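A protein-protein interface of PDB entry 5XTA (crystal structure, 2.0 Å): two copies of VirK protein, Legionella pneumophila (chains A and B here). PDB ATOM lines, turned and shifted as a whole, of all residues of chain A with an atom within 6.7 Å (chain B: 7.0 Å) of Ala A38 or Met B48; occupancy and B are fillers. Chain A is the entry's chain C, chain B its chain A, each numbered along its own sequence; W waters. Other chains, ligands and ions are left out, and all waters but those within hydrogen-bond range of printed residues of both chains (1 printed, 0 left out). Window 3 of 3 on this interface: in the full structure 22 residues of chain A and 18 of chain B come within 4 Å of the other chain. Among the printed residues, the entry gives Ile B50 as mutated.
The backbone carbonyl oxygen (O) of Val B47 lies within hydrogen-bond range of the backbone NH (N) of Ser A41, at 3.0 Å. The backbone NH of Ile A39 is in hydrogen-bond range of the backbone carbonyl oxygen of Val B49, 2.8 Å away. The backbone NH (N) of Gly B51 sits at hydrogen-bond distance from the backbone carbonyl oxygen (O) of Ser A37 (3.0 Å).
The backbone carbonyl oxygen (O) of Met B48 sits at hydrogen-bond distance from the backbone NH (N) of Thr B56 (2.9 Å). O of Val A40 sits at hydrogen-bond distance from N of Ile A24 (2.6 Å). N of Leu A26 is in hydrogen-bond range of O of Ala A38, at 3.1 Å.
Ala A38 touches Met B48 (CB to CE, 3.7 Å). Ala A38 touches Val B49. O of Ile A39 touches CA of Met B48 (3.2 Å). CA of Val A40 touches O of Val B47, at 3.7 Å. Val A40 touches Met B48. Ser A41 touches Ile B14 (CB to CG2, 3.95 Å). Ala B46 touches Ser A41 (CA to O, 3.1 Å).
Ala A38 touches just these residues of chain B: Met B48 (3.7 Å) and Val B49 (3.1 Å). Met B48 touches just these residues of chain A: Ala A38 (3.7 Å), Ile A39 (3.2 Å) and Val A40 (3.8 Å). Of the printed residues of chain B, Ser A41 touches Ile B14, Ala B46 and Val B47. Printed residues of chain B within 4 Å of Ser A37: Gly B51 (3.0 Å). Of the printed residues of chain A, Val B47 touches Val A40 (3.7 Å) and Ser A41 (3.0 Å). The nearest residue of chain A that does not touch Met B48 is Ser A41 (5.1 Å). The nearest printed residue of chain A that does not touch Ala B46 is Val A40 (6.0 Å).
Of the 12 printed residues of chain B, 6 touch a printed residue of chain A. Hydrophobic or aromatic side chains of chain B within 4 Å of the printed part of chain A: Ile B14, Ala B46 and Met B48. Hydrophobic or aromatic side chains of chain A within 4 Å of the printed part of chain B: Ala A38 and Val A40. Among the printed residues, no Asp or Glu carboxylate lies within 4 Å of a Lys or Arg side-chain nitrogen of the other chain.
No position is printed for both chains. Of the 10 pairs that touch across the chains among the printed residues, none has its exchanged pair printed and touching as well.
Water W1 lies within hydrogen-bond range of OG of Ser A41 (2.6 Å) and O of Ile B14 (2.8 Å).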
ATOM      1  N   ILE A  24       0.964  -8.441   7.756  1.00  0.00           N
ATOM      2  CA  ILE A  24       1.673  -8.563   8.979  1.00  0.00           C
ATOM      3  C   ILE A  24       2.470  -9.849   8.966  1.00  0.00           C
ATOM      4  O   ILE A  24       1.920 -10.937   8.743  1.00  0.00           O
ATOM      5  CB  ILE A  24       0.759  -8.576  10.231  1.00  0.00           C
ATOM      6  CG1 ILE A  24      -0.432  -7.599  10.147  1.00  0.00           C
ATOM      7  CG2 ILE A  24       1.613  -8.406  11.483  1.00  0.00           C
ATOM      8  CD1 ILE A  24      -0.144  -6.209  10.465  1.00  0.00           C
ATOM      9  N   ASN A  25       3.752  -9.730   9.267  1.00  0.00           N
ATOM     10  CA  ASN A  25       4.658 -10.883   9.382  1.00  0.00           C
ATOM     11  C   ASN A  25       4.946 -11.052  10.833  1.00  0.00           C
ATOM     12  O   ASN A  25       5.789 -10.365  11.391  1.00  0.00           O
ATOM     13  CB  ASN A  25       5.937 -10.651   8.570  1.00  0.00           C
ATOM     14  CG  ASN A  25       6.809 -11.896   8.435  1.00  0.00           C
ATOM     15  OD1 ASN A  25       6.619 -12.897   9.117  1.00  0.00           O
ATOM     16  ND2 ASN A  25       7.766 -11.829   7.521  1.00  0.00           N
ATOM     17  N   LEU A  26       4.197 -11.949  11.442  1.00  0.00           N
ATOM     18  CA  LEU A  26       4.207 -12.184  12.882  1.00  0.00           C
ATOM     19  C   LEU A  26       5.555 -12.501  13.492  1.00  0.00           C
ATOM     20  O   LEU A  26       5.803 -12.122  14.639  1.00  0.00           O
ATOM     21  CB  LEU A  26       3.259 -13.316  13.234  1.00  0.00           C
ATOM     22  CG  LEU A  26       1.804 -12.964  13.534  1.00  0.00           C
ATOM     23  CD1 LEU A  26       1.193 -11.891  12.661  1.00  0.00           C
ATOM     24  CD2 LEU A  26       0.973 -14.231  13.464  1.00  0.00           C
ATOM     25  N   LYS A  27       6.417 -13.183  12.743  1.00  0.00           N
ATOM     26  CA  LYS A  27       7.722 -13.552  13.260  1.00  0.00           C
ATOM     27  C   LYS A  27       8.647 -12.331  13.360  1.00  0.00           C
ATOM     28  O   LYS A  27       9.648 -12.398  14.030  1.00  0.00           O
ATOM     29  CB  LYS A  27       8.359 -14.678  12.441  1.00  0.00           C
ATOM     30  CG  LYS A  27       9.006 -14.248  11.143  1.00  0.00           C
ATOM     31  CD  LYS A  27       9.608 -15.434  10.405  1.00  0.00           C
ATOM     32  CE  LYS A  27      10.732 -15.011   9.452  1.00  0.00           C
ATOM     33  NZ  LYS A  27      10.240 -14.517   8.135  1.00  0.00           N
ATOM     34  N   LEU A  35       3.978 -16.202  18.970  1.00  0.00           N
ATOM     35  CA  LEU A  35       2.957 -16.525  17.968  1.00  0.00           C
ATOM     36  C   LEU A  35       3.662 -17.296  16.871  1.00  0.00           C
ATOM     37  O   LEU A  35       4.798 -16.971  16.514  1.00  0.00           O
ATOM     38  CB  LEU A  35       2.312 -15.264  17.375  1.00  0.00           C
ATOM     39  CG  LEU A  35       2.664 -13.896  17.984  1.00  0.00           C
ATOM     40  CD1 LEU A  35       3.813 -13.199  17.244  1.00  0.00           C
ATOM     41  CD2 LEU A  35       1.456 -13.000  18.007  1.00  0.00           C
ATOM     42  N   ASN A  36       2.995 -18.311  16.333  1.00  0.00           N
ATOM     43  CA  ASN A  36       3.580 -19.104  15.260  1.00  0.00           C
ATOM     44  C   ASN A  36       3.710 -18.310  13.991  1.00  0.00           C
ATOM     45  O   ASN A  36       2.868 -17.470  13.666  1.00  0.00           O
ATOM     46  CB  ASN A  36       2.784 -20.366  15.012  1.00  0.00           C
ATOM     47  CG  ASN A  36       2.888 -21.318  16.168  1.00  0.00           C
ATOM     48  OD1 ASN A  36       1.996 -21.369  17.029  1.00  0.00           O
ATOM     49  ND2 ASN A  36       4.006 -22.019  16.253  1.00  0.00           N
ATOM     50  N   SER A  37       4.795 -18.594  13.291  1.00  0.00           N
ATOM     51  CA  SER A  37       5.161 -17.873  12.095  1.00  0.00           C
ATOM     52  C   SER A  37       4.006 -17.946  11.079  1.00  0.00           C
ATOM     53  O   SER A  37       3.526 -19.018  10.716  1.00  0.00           O
ATOM     54  CB  SER A  37       6.471 -18.424  11.536  1.00  0.00           C
ATOM     55  OG  SER A  37       6.699 -17.981  10.215  1.00  0.00           O
ATOM     56  N   ALA A  38       3.518 -16.777  10.715  1.00  0.00           N
ATOM     57  CA  ALA A  38       2.439 -16.659   9.765  1.00  0.00           C
ATOM     58  C   ALA A  38       2.517 -15.275   9.185  1.00  0.00           C
ATOM     59  O   ALA A  38       3.070 -14.331   9.791  1.00  0.00           O
ATOM     60  CB  ALA A  38       1.087 -16.871  10.435  1.00  0.00           C
ATOM     61  N   ILE A  39       1.981 -15.161   7.995  1.00  0.00           N
ATOM     62  CA  ILE A  39       1.782 -13.898   7.373  1.00  0.00           C
ATOM     63  C   ILE A  39       0.291 -13.700   7.365  1.00  0.00           C
ATOM     64  O   ILE A  39      -0.428 -14.593   6.960  1.00  0.00           O
ATOM     65  CB  ILE A  39       2.285 -13.905   5.913  1.00  0.00           C
ATOM     66  CG1 ILE A  39       3.770 -14.339   5.822  1.00  0.00           C
ATOM     67  CG2 ILE A  39       2.020 -12.559   5.271  1.00  0.00           C
ATOM     68  CD1 ILE A  39       4.761 -13.336   6.347  1.00  0.00           C
ATOM     69  N   VAL A  40      -0.168 -12.515   7.755  1.00  0.00           N
ATOM     70  CA  VAL A  40      -1.599 -12.197   7.825  1.00  0.00           C
ATOM     71  C   VAL A  40      -1.859 -10.920   7.050  1.00  0.00           C
ATOM     72  O   VAL A  40      -1.185  -9.907   7.262  1.00  0.00           O
ATOM     73  CB  VAL A  40      -2.022 -11.957   9.280  1.00  0.00           C
ATOM     74  CG1 VAL A  40      -3.497 -11.607   9.385  1.00  0.00           C
ATOM     75  CG2 VAL A  40      -1.728 -13.197  10.085  1.00  0.00           C
ATOM     76  N   SER A  41      -2.833 -10.997   6.156  1.00  0.00           N
ATOM     77  CA  SER A  41      -3.246  -9.911   5.315  1.00  0.00           C
ATOM     78  C   SER A  41      -4.709  -9.616   5.608  1.00  0.00           C
ATOM     79  O   SER A  41      -5.553 -10.527   5.631  1.00  0.00           O
ATOM     80  CB  SER A  41      -3.119 -10.285   3.846  1.00  0.00           C
ATOM     81  OG  SER A  41      -3.784  -9.320   3.027  1.00  0.00           O
ATOM     82  N   ILE B  14      -0.026 -12.694  -1.577  1.00  0.00           N
ATOM     83  CA  ILE B  14      -0.469 -12.317  -0.243  1.00  0.00           C
ATOM     84  C   ILE B  14       0.551 -11.356   0.396  1.00  0.00           C
ATOM     85  O   ILE B  14       0.193 -10.274   0.910  1.00  0.00           O
ATOM     86  CB  ILE B  14      -0.725 -13.551   0.629  1.00  0.00           C
ATOM     87  CG1 ILE B  14      -1.888 -14.348   0.058  1.00  0.00           C
ATOM     88  CG2 ILE B  14      -1.018 -13.138   2.089  1.00  0.00           C
ATOM     89  CD1 ILE B  14      -1.963 -15.757   0.570  1.00  0.00           C
ATOM     90  N   ALA B  46      -9.587 -11.107   4.329  1.00  0.00           N
ATOM     91  CA  ALA B  46      -8.437 -11.558   5.119  1.00  0.00           C
ATOM     92  C   ALA B  46      -7.995 -12.973   4.717  1.00  0.00           C
ATOM     93  O   ALA B  46      -8.799 -13.810   4.318  1.00  0.00           O
ATOM     94  CB  ALA B  46      -8.789 -11.548   6.592  1.00  0.00           C
ATOM     95  N   VAL B  47      -6.692 -13.215   4.789  1.00  0.00           N
ATOM     96  CA  VAL B  47      -6.102 -14.483   4.358  1.00  0.00           C
ATOM     97  C   VAL B  47      -4.758 -14.591   5.089  1.00  0.00           C
ATOM     98  O   VAL B  47      -4.143 -13.557   5.484  1.00  0.00           O
ATOM     99  CB  VAL B  47      -5.983 -14.546   2.805  1.00  0.00           C
ATOM    100  CG1 VAL B  47      -5.107 -13.430   2.294  1.00  0.00           C
ATOM    101  CG2 VAL B  47      -5.459 -15.885   2.305  1.00  0.00           C
ATOM    102  N   MET B  48      -4.312 -15.824   5.271  1.00  0.00           N
ATOM    103  CA  MET B  48      -3.096 -16.077   6.052  1.00  0.00           C
ATOM    104  C   MET B  48      -2.264 -17.102   5.373  1.00  0.00           C
ATOM    105  O   MET B  48      -2.808 -18.000   4.748  1.00  0.00           O
ATOM    106  CB  MET B  48      -3.333 -16.684   7.414  1.00  0.00           C
ATOM    107  CG  MET B  48      -4.444 -16.039   8.192  1.00  0.00           C
ATOM    108  SD  MET B  48      -4.487 -16.739  10.057  1.00  0.00           S
ATOM    109  CE  MET B  48      -2.574 -16.883  10.545  1.00  0.00           C
ATOM    110  N   VAL B  49      -0.944 -16.973   5.531  1.00  0.00           N
ATOM    111  CA  VAL B  49       0.005 -18.007   5.154  1.00  0.00           C
ATOM    112  C   VAL B  49       0.610 -18.516   6.449  1.00  0.00           C
ATOM    113  O   VAL B  49       1.139 -17.727   7.206  1.00  0.00           O
ATOM    114  CB  VAL B  49       1.112 -17.454   4.272  1.00  0.00           C
ATOM    115  CG1 VAL B  49       2.029 -18.580   3.813  1.00  0.00           C
ATOM    116  CG2 VAL B  49       0.510 -16.722   3.069  1.00  0.00           C
ATOM    117  N   ILE B  50       0.444 -19.808   6.713  1.00  0.00           N
ATOM    118  CA  ILE B  50       0.931 -20.448   7.926  1.00  0.00           C
ATOM    119  C   ILE B  50       2.213 -21.188   7.584  1.00  0.00           C
ATOM    120  O   ILE B  50       2.203 -22.086   6.728  1.00  0.00           O
ATOM    121  CB  ILE B  50      -0.032 -21.495   8.500  1.00  0.00           C
ATOM    122  CG1 ILE B  50      -1.469 -20.999   8.534  1.00  0.00           C
ATOM    123  CG2 ILE B  50       0.423 -21.919   9.899  1.00  0.00           C
ATOM    124  CD1 ILE B  50      -1.669 -19.828   9.450  1.00  0.00           C
ATOM    125  N   GLY B  51       3.297 -20.813   8.261  1.00  0.00           N
ATOM    126  CA  GLY B  51       4.618 -21.376   7.979  1.00  0.00           C
ATOM    127  C   GLY B  51       4.873 -20.927   6.559  1.00  0.00           C
ATOM    128  O   GLY B  51       4.455 -19.834   6.171  1.00  0.00           O
ATOM    129  N   ARG B  54       0.980 -23.587   4.242  1.00  0.00           N
ATOM    130  CA  ARG B  54      -0.479 -23.574   4.160  1.00  0.00           C
ATOM    131  C   ARG B  54      -0.969 -22.155   3.963  1.00  0.00           C
ATOM    132  O   ARG B  54      -0.422 -21.228   4.571  1.00  0.00           O
ATOM    133  CB  ARG B  54      -1.097 -24.119   5.465  1.00  0.00           C
ATOM    134  CG  ARG B  54      -1.482 -25.569   5.430  1.00  0.00           C
ATOM    135  CD  ARG B  54      -2.270 -26.006   6.667  1.00  0.00           C
ATOM    136  NE  ARG B  54      -1.801 -25.465   7.957  1.00  0.00           N
ATOM    137  CZ  ARG B  54      -2.562 -24.917   8.919  1.00  0.00           C
ATOM    138  NH1 ARG B  54      -3.879 -24.758   8.789  1.00  0.00           N
ATOM    139  NH2 ARG B  54      -1.988 -24.511  10.052  1.00  0.00           N
ATOM    140  N   VAL B  55      -2.012 -22.007   3.138  1.00  0.00           N
ATOM    141  CA  VAL B  55      -2.778 -20.773   3.016  1.00  0.00           C
ATOM    142  C   VAL B  55      -4.173 -21.036   3.523  1.00  0.00           C
ATOM    143  O   VAL B  55      -4.823 -22.032   3.117  1.00  0.00           O
ATOM    144  CB  VAL B  55      -2.889 -20.333   1.552  1.00  0.00           C
ATOM    145  CG1 VAL B  55      -3.851 -19.161   1.379  1.00  0.00           C
ATOM    146  CG2 VAL B  55      -1.526 -19.972   1.007  1.00  0.00           C
ATOM    147  N   THR B  56      -4.671 -20.136   4.383  1.00  0.00           N
ATOM    148  CA  THR B  56      -6.005 -20.307   4.924  1.00  0.00           C
ATOM    149  C   THR B  56      -6.797 -19.038   4.891  1.00  0.00           C
ATOM    150  O   THR B  56      -6.256 -17.943   4.918  1.00  0.00           O
ATOM    151  CB  THR B  56      -5.990 -20.820   6.380  1.00  0.00           C
ATOM    152  OG1 THR B  56      -5.442 -19.810   7.234  1.00  0.00           O
ATOM    153  CG2 THR B  56      -5.153 -22.045   6.504  1.00  0.00           C
ATOM    154  N   ALA B  57      -8.097 -19.203   4.790  1.00  0.00           N
ATOM    155  CA  ALA B  57      -9.025 -18.070   4.797  1.00  0.00           C
ATOM    156  C   ALA B  57     -10.374 -18.592   5.113  1.00  0.00           C
ATOM    157  O   ALA B  57     -10.577 -19.783   5.094  1.00  0.00           O
ATOM    158  CB  ALA B  57      -9.059 -17.370   3.450  1.00  0.00           C
ATOM    159  N   LYS B  79     -14.430 -22.620   5.600  1.00  0.00           N
ATOM    160  CA  LYS B  79     -13.009 -22.551   5.903  1.00  0.00           C
ATOM    161  C   LYS B  79     -12.198 -23.150   4.726  1.00  0.00           C
ATOM    162  O   LYS B  79     -12.430 -24.278   4.320  1.00  0.00           O
ATOM    163  CB  LYS B  79     -12.780 -23.306   7.212  1.00  0.00           C
ATOM    164  CG  LYS B  79     -11.334 -23.495   7.635  1.00  0.00           C
ATOM    165  CD  LYS B  79     -10.714 -22.193   8.056  1.00  0.00           C
ATOM    166  CE  LYS B  79      -9.296 -22.449   8.549  1.00  0.00           C
ATOM    167  NZ  LYS B  79      -8.579 -21.177   8.740  1.00  0.00           N
HETATM  168  O   HOH W   1      -2.495  -9.477   0.720  1.00  0.00           O
